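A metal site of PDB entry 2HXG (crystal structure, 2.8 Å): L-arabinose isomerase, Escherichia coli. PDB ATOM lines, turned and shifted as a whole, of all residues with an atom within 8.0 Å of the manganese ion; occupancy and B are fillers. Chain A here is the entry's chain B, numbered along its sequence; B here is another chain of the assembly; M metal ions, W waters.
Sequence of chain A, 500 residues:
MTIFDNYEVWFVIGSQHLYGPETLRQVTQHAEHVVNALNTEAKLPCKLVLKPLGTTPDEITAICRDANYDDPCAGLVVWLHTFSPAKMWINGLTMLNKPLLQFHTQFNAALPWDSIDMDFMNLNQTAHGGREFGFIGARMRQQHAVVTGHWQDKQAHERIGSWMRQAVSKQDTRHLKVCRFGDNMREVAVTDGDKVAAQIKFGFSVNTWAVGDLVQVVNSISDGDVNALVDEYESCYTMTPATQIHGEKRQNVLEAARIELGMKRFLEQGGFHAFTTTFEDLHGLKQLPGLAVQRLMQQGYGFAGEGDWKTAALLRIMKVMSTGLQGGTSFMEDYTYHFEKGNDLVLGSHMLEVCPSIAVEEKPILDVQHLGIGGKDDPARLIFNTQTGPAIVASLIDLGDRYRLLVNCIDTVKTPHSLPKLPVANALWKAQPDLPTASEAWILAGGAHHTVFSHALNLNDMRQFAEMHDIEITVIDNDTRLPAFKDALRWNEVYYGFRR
The manganese ion is bound by the side-chain carboxylate (OE1) of Glu 306 (2.0 Å), a ring nitrogen (NE2) of His 350 (2.1 Å), the side-chain carboxylate (OE2) of Glu 333 (2.2 Å) and water W1 (2.5 Å).
Slightly farther from the manganese ion lies water W2 (2.8 Å).
Slightly farther from the manganese ion lies NE2 of His 450 (2.8 Å).
NE2 of His 450 sits close to OE1 of Glu 306 (3.4 Å).
A ring nitrogen (NE2) of His 450 sits close to a ring nitrogen (NE2) of His 350 (3.2 Å).
ND1 of His 350 lies within hydrogen-bond range of OE1 of Glu 353, 3.2 Å away.
OE2 of Glu 333 lies close to NE2 of His 450, 3.3 Å away.
OE2 of Glu 333 lies close to ND1 of His 449 (3.1 Å).
The side-chain carboxylate of Glu 333 sits at hydrogen-bond distance from a ring nitrogen (ND1) of His 128 of chain B, at 3.2 Å.
The backbone carbonyl oxygen (O) of Glu 333 sits at hydrogen-bond distance from the backbone NH (N) of Ser 349.
ND1 of His 450 lies within hydrogen-bond range of OD2 of Asp 308.
Of the 21 residues printed, 4 come within 4 Å of the manganese ion.
The nearest printed residue that does not touch the manganese ion is His 449 (4.6 Å).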
ATOM      1  N   MET A 185       7.573   8.235   9.141  1.00  0.00           N
ATOM      2  CA  MET A 185       7.232   9.621   9.392  1.00  0.00           C
ATOM      3  C   MET A 185       7.151   9.814  10.902  1.00  0.00           C
ATOM      4  O   MET A 185       6.509   9.023  11.584  1.00  0.00           O
ATOM      5  CB  MET A 185       5.877   9.969   8.749  1.00  0.00           C
ATOM      6  CG  MET A 185       5.609  11.478   8.597  1.00  0.00           C
ATOM      7  SD  MET A 185       3.931  11.912   8.064  1.00  0.00           S
ATOM      8  CE  MET A 185       3.842  11.013   6.548  1.00  0.00           C
ATOM      9  N   THR A 191       1.393   3.323  11.114  1.00  0.00           N
ATOM     10  CA  THR A 191       2.442   2.777  10.263  1.00  0.00           C
ATOM     11  C   THR A 191       3.599   2.178  11.085  1.00  0.00           C
ATOM     12  O   THR A 191       4.517   1.562  10.537  1.00  0.00           O
ATOM     13  CB  THR A 191       3.008   3.854   9.368  1.00  0.00           C
ATOM     14  OG1 THR A 191       3.541   4.896  10.192  1.00  0.00           O
ATOM     15  CG2 THR A 191       1.910   4.427   8.467  1.00  0.00           C
ATOM     16  N   PHE A 279       9.742  10.878   3.144  1.00  0.00           N
ATOM     17  CA  PHE A 279      10.067  12.191   2.594  1.00  0.00           C
ATOM     18  C   PHE A 279      10.901  13.034   3.570  1.00  0.00           C
ATOM     19  O   PHE A 279      11.464  14.074   3.182  1.00  0.00           O
ATOM     20  CB  PHE A 279       8.801  12.940   2.138  1.00  0.00           C
ATOM     21  CG  PHE A 279       7.856  13.282   3.244  1.00  0.00           C
ATOM     22  CD1 PHE A 279       8.170  14.250   4.183  1.00  0.00           C
ATOM     23  CD2 PHE A 279       6.631  12.647   3.329  1.00  0.00           C
ATOM     24  CE1 PHE A 279       7.302  14.569   5.192  1.00  0.00           C
ATOM     25  CE2 PHE A 279       5.750  12.948   4.340  1.00  0.00           C
ATOM     26  CZ  PHE A 279       6.088  13.916   5.284  1.00  0.00           C
ATOM     27  N   ALA A 304       4.716   1.106   0.281  1.00  0.00           N
ATOM     28  CA  ALA A 304       3.888   2.079   0.958  1.00  0.00           C
ATOM     29  C   ALA A 304       4.696   3.332   1.313  1.00  0.00           C
ATOM     30  O   ALA A 304       5.915   3.277   1.496  1.00  0.00           O
ATOM     31  CB  ALA A 304       3.237   1.477   2.197  1.00  0.00           C
ATOM     32  N   GLY A 305       3.996   4.441   1.402  1.00  0.00           N
ATOM     33  CA  GLY A 305       4.619   5.714   1.689  1.00  0.00           C
ATOM     34  C   GLY A 305       5.097   5.820   3.112  1.00  0.00           C
ATOM     35  O   GLY A 305       4.781   4.989   3.948  1.00  0.00           O
ATOM     36  N   GLU A 306       5.871   6.870   3.367  1.00  0.00           N
ATOM     37  CA  GLU A 306       6.308   7.244   4.707  1.00  0.00           C
ATOM     38  C   GLU A 306       6.541   6.074   5.692  1.00  0.00           C
ATOM     39  O   GLU A 306       5.907   6.003   6.749  1.00  0.00           O
ATOM     40  CB  GLU A 306       5.362   8.314   5.292  1.00  0.00           C
ATOM     41  CG  GLU A 306       3.861   8.062   5.091  1.00  0.00           C
ATOM     42  CD  GLU A 306       3.217   9.016   4.112  1.00  0.00           C
ATOM     43  OE1 GLU A 306       1.990   9.241   4.189  1.00  0.00           O
ATOM     44  OE2 GLU A 306       3.943   9.578   3.272  1.00  0.00           O
ATOM     45  N   ASP A 308       5.911   2.895   5.901  1.00  0.00           N
ATOM     46  CA  ASP A 308       4.797   2.017   6.301  1.00  0.00           C
ATOM     47  C   ASP A 308       4.997   0.570   5.840  1.00  0.00           C
ATOM     48  O   ASP A 308       4.444   0.129   4.831  1.00  0.00           O
ATOM     49  CB  ASP A 308       3.480   2.597   5.756  1.00  0.00           C
ATOM     50  CG  ASP A 308       2.272   1.755   6.127  1.00  0.00           C
ATOM     51  OD1 ASP A 308       2.411   0.751   6.876  1.00  0.00           O
ATOM     52  OD2 ASP A 308       1.165   2.102   5.664  1.00  0.00           O
ATOM     53  N   PHE A 331      -1.312   0.403  -3.749  1.00  0.00           N
ATOM     54  CA  PHE A 331      -1.275   1.299  -2.598  1.00  0.00           C
ATOM     55  C   PHE A 331      -2.218   2.509  -2.811  1.00  0.00           C
ATOM     56  O   PHE A 331      -2.439   2.948  -3.941  1.00  0.00           O
ATOM     57  CB  PHE A 331       0.168   1.771  -2.404  1.00  0.00           C
ATOM     58  CG  PHE A 331       0.329   2.802  -1.342  1.00  0.00           C
ATOM     59  CD1 PHE A 331       0.034   2.509  -0.040  1.00  0.00           C
ATOM     60  CD2 PHE A 331       0.777   4.066  -1.653  1.00  0.00           C
ATOM     61  CE1 PHE A 331       0.183   3.459   0.932  1.00  0.00           C
ATOM     62  CE2 PHE A 331       0.928   5.009  -0.674  1.00  0.00           C
ATOM     63  CZ  PHE A 331       0.628   4.713   0.612  1.00  0.00           C
ATOM     64  N   MET A 332      -2.778   3.030  -1.707  1.00  0.00           N
ATOM     65  CA  MET A 332      -3.911   3.959  -1.773  1.00  0.00           C
ATOM     66  C   MET A 332      -4.171   4.714  -0.469  1.00  0.00           C
ATOM     67  O   MET A 332      -4.353   4.090   0.577  1.00  0.00           O
ATOM     68  CB  MET A 332      -5.178   3.159  -2.113  1.00  0.00           C
ATOM     69  CG  MET A 332      -6.414   4.002  -2.444  1.00  0.00           C
ATOM     70  SD  MET A 332      -6.157   5.085  -3.839  1.00  0.00           S
ATOM     71  CE  MET A 332      -5.710   3.898  -5.091  1.00  0.00           C
ATOM     72  N   GLU A 333      -4.235   6.049  -0.539  1.00  0.00           N
ATOM     73  CA  GLU A 333      -4.668   6.867   0.605  1.00  0.00           C
ATOM     74  C   GLU A 333      -6.029   7.494   0.314  1.00  0.00           C
ATOM     75  O   GLU A 333      -6.260   8.014  -0.776  1.00  0.00           O
ATOM     76  CB  GLU A 333      -3.643   7.973   0.947  1.00  0.00           C
ATOM     77  CG  GLU A 333      -3.734   8.527   2.381  1.00  0.00           C
ATOM     78  CD  GLU A 333      -2.478   9.267   2.841  1.00  0.00           C
ATOM     79  OE1 GLU A 333      -2.282  10.423   2.405  1.00  0.00           O
ATOM     80  OE2 GLU A 333      -1.704   8.700   3.656  1.00  0.00           O
ATOM     81  N   ASP A 334      -6.915   7.457   1.313  1.00  0.00           N
ATOM     82  CA  ASP A 334      -8.236   8.071   1.197  1.00  0.00           C
ATOM     83  C   ASP A 334      -8.065   9.589   1.291  1.00  0.00           C
ATOM     84  O   ASP A 334      -7.965  10.125   2.398  1.00  0.00           O
ATOM     85  CB  ASP A 334      -9.167   7.560   2.300  1.00  0.00           C
ATOM     86  CG  ASP A 334      -9.207   6.052   2.369  1.00  0.00           C
ATOM     87  OD1 ASP A 334     -10.287   5.461   2.164  1.00  0.00           O
ATOM     88  OD2 ASP A 334      -8.140   5.453   2.629  1.00  0.00           O
ATOM     89  N   TYR A 335      -8.053  10.262   0.141  1.00  0.00           N
ATOM     90  CA  TYR A 335      -7.501  11.613   0.051  1.00  0.00           C
ATOM     91  C   TYR A 335      -8.519  12.735   0.247  1.00  0.00           C
ATOM     92  O   TYR A 335      -8.197  13.768   0.838  1.00  0.00           O
ATOM     93  CB  TYR A 335      -6.717  11.794  -1.263  1.00  0.00           C
ATOM     94  CG  TYR A 335      -5.358  12.469  -1.114  1.00  0.00           C
ATOM     95  CD1 TYR A 335      -4.569  12.257   0.019  1.00  0.00           C
ATOM     96  CD2 TYR A 335      -4.836  13.283  -2.134  1.00  0.00           C
ATOM     97  CE1 TYR A 335      -3.329  12.852   0.165  1.00  0.00           C
ATOM     98  CE2 TYR A 335      -3.564  13.893  -2.000  1.00  0.00           C
ATOM     99  CZ  TYR A 335      -2.819  13.649  -0.824  1.00  0.00           C
ATOM    100  OH  TYR A 335      -1.559  14.180  -0.559  1.00  0.00           O
ATOM    101  N   SER A 349      -5.746   8.446  -3.503  1.00  0.00           N
ATOM    102  CA  SER A 349      -4.444   8.820  -4.112  1.00  0.00           C
ATOM    103  C   SER A 349      -3.352   8.851  -3.034  1.00  0.00           C
ATOM    104  O   SER A 349      -3.585   8.480  -1.892  1.00  0.00           O
ATOM    105  CB  SER A 349      -4.528  10.199  -4.817  1.00  0.00           C
ATOM    106  OG  SER A 349      -3.281  10.576  -5.387  1.00  0.00           O
ATOM    107  N   HIS A 350      -2.158   9.286  -3.423  1.00  0.00           N
ATOM    108  CA  HIS A 350      -1.101   9.687  -2.476  1.00  0.00           C
ATOM    109  C   HIS A 350      -0.458  10.945  -3.118  1.00  0.00           C
ATOM    110  O   HIS A 350      -0.986  11.456  -4.114  1.00  0.00           O
ATOM    111  CB  HIS A 350      -0.078   8.571  -2.288  1.00  0.00           C
ATOM    112  CG  HIS A 350       0.468   8.462  -0.900  1.00  0.00           C
ATOM    113  ND1 HIS A 350       1.713   8.939  -0.551  1.00  0.00           N
ATOM    114  CD2 HIS A 350      -0.052   7.896   0.220  1.00  0.00           C
ATOM    115  CE1 HIS A 350       1.929   8.681   0.732  1.00  0.00           C
ATOM    116  NE2 HIS A 350       0.880   8.055   1.225  1.00  0.00           N
ATOM    117  N   MET A 351       0.652  11.418  -2.558  1.00  0.00           N
ATOM    118  CA  MET A 351       1.442  12.504  -3.181  1.00  0.00           C
ATOM    119  C   MET A 351       1.790  12.185  -4.629  1.00  0.00           C
ATOM    120  O   MET A 351       1.745  13.064  -5.495  1.00  0.00           O
ATOM    121  CB  MET A 351       2.792  12.708  -2.472  1.00  0.00           C
ATOM    122  CG  MET A 351       2.790  12.791  -0.955  1.00  0.00           C
ATOM    123  SD  MET A 351       4.493  12.701  -0.412  1.00  0.00           S
ATOM    124  CE  MET A 351       4.532  11.006   0.129  1.00  0.00           C
ATOM    125  N   GLU A 353       2.613   8.125  -5.426  1.00  0.00           N
ATOM    126  CA  GLU A 353       2.804   6.681  -5.603  1.00  0.00           C
ATOM    127  C   GLU A 353       1.518   5.867  -5.817  1.00  0.00           C
ATOM    128  O   GLU A 353       1.120   5.100  -4.959  1.00  0.00           O
ATOM    129  CB  GLU A 353       3.578   6.125  -4.397  1.00  0.00           C
ATOM    130  CG  GLU A 353       4.884   6.875  -4.064  1.00  0.00           C
ATOM    131  CD  GLU A 353       4.731   7.893  -2.965  1.00  0.00           C
ATOM    132  OE1 GLU A 353       3.757   8.676  -2.990  1.00  0.00           O
ATOM    133  OE2 GLU A 353       5.600   7.907  -2.064  1.00  0.00           O
ATOM    134  N   HIS A 449      -5.191   5.106   7.355  1.00  0.00           N
ATOM    135  CA  HIS A 449      -5.406   5.893   6.129  1.00  0.00           C
ATOM    136  C   HIS A 449      -4.725   5.240   4.921  1.00  0.00           C
ATOM    137  O   HIS A 449      -5.082   5.516   3.785  1.00  0.00           O
ATOM    138  CB  HIS A 449      -4.864   7.299   6.287  1.00  0.00           C
ATOM    139  CG  HIS A 449      -3.504   7.351   6.915  1.00  0.00           C
ATOM    140  ND1 HIS A 449      -2.347   7.097   6.209  1.00  0.00           N
ATOM    141  CD2 HIS A 449      -3.116   7.617   8.182  1.00  0.00           C
ATOM    142  CE1 HIS A 449      -1.302   7.215   7.012  1.00  0.00           C
ATOM    143  NE2 HIS A 449      -1.739   7.538   8.221  1.00  0.00           N
ATOM    144  N   HIS A 450      -3.715   4.414   5.196  1.00  0.00           N
ATOM    145  CA  HIS A 450      -3.047   3.611   4.166  1.00  0.00           C
ATOM    146  C   HIS A 450      -3.813   2.338   3.921  1.00  0.00           C
ATOM    147  O   HIS A 450      -4.174   1.668   4.876  1.00  0.00           O
ATOM    148  CB  HIS A 450      -1.617   3.274   4.571  1.00  0.00           C
ATOM    149  CG  HIS A 450      -0.643   4.400   4.341  1.00  0.00           C
ATOM    150  ND1 HIS A 450       0.651   4.359   4.800  1.00  0.00           N
ATOM    151  CD2 HIS A 450      -0.784   5.579   3.708  1.00  0.00           C
ATOM    152  CE1 HIS A 450       1.273   5.471   4.459  1.00  0.00           C
ATOM    153  NE2 HIS A 450       0.418   6.233   3.797  1.00  0.00           N
ATOM    154  N   PHE B  83      -4.122  16.081   8.376  1.00  0.00           N
ATOM    155  CA  PHE B  83      -3.346  15.013   9.029  1.00  0.00           C
ATOM    156  C   PHE B  83      -2.639  15.578  10.262  1.00  0.00           C
ATOM    157  O   PHE B  83      -1.998  16.635  10.210  1.00  0.00           O
ATOM    158  CB  PHE B  83      -2.319  14.407   8.067  1.00  0.00           C
ATOM    159  CG  PHE B  83      -1.773  13.097   8.484  1.00  0.00           C
ATOM    160  CD1 PHE B  83      -0.417  12.915   8.692  1.00  0.00           C
ATOM    161  CD2 PHE B  83      -2.614  11.998   8.645  1.00  0.00           C
ATOM    162  CE1 PHE B  83       0.109  11.661   9.083  1.00  0.00           C
ATOM    163  CE2 PHE B  83      -2.120  10.737   9.028  1.00  0.00           C
ATOM    164  CZ  PHE B  83      -0.738  10.566   9.251  1.00  0.00           C
ATOM    165  N   GLN B 125      -7.465  17.611   4.758  1.00  0.00           N
ATOM    166  CA  GLN B 125      -7.027  16.219   4.726  1.00  0.00           C
ATOM    167  C   GLN B 125      -7.862  15.260   5.579  1.00  0.00           C
ATOM    168  O   GLN B 125      -7.536  14.066   5.671  1.00  0.00           O
ATOM    169  CB  GLN B 125      -5.555  16.115   5.141  1.00  0.00           C
ATOM    170  CG  GLN B 125      -4.607  16.912   4.272  1.00  0.00           C
ATOM    171  CD  GLN B 125      -3.224  16.300   4.203  1.00  0.00           C
ATOM    172  OE1 GLN B 125      -2.677  16.085   3.117  1.00  0.00           O
ATOM    173  NE2 GLN B 125      -2.655  15.988   5.366  1.00  0.00           N
ATOM    174  N   HIS B 128      -7.920  11.218   5.424  1.00  0.00           N
ATOM    175  CA  HIS B 128      -6.830  10.382   5.980  1.00  0.00           C
ATOM    176  C   HIS B 128      -6.495  10.733   7.440  1.00  0.00           C
ATOM    177  O   HIS B 128      -6.161   9.849   8.230  1.00  0.00           O
ATOM    178  CB  HIS B 128      -5.562  10.307   5.085  1.00  0.00           C
ATOM    179  CG  HIS B 128      -5.151  11.578   4.415  1.00  0.00           C
ATOM    180  ND1 HIS B 128      -3.915  12.153   4.616  1.00  0.00           N
ATOM    181  CD2 HIS B 128      -5.765  12.351   3.479  1.00  0.00           C
ATOM    182  CE1 HIS B 128      -3.804  13.245   3.886  1.00  0.00           C
ATOM    183  NE2 HIS B 128      -4.917  13.385   3.176  1.00  0.00           N
HETATM  184 MN    MN M   1       0.410   8.936   3.016  1.00  0.00          MN
HETATM  185  O   HOH W   1      -0.381   9.943   5.129  1.00  0.00           O
HETATM  186  O   HOH W   2       0.086  11.595   3.660  1.00  0.00           O
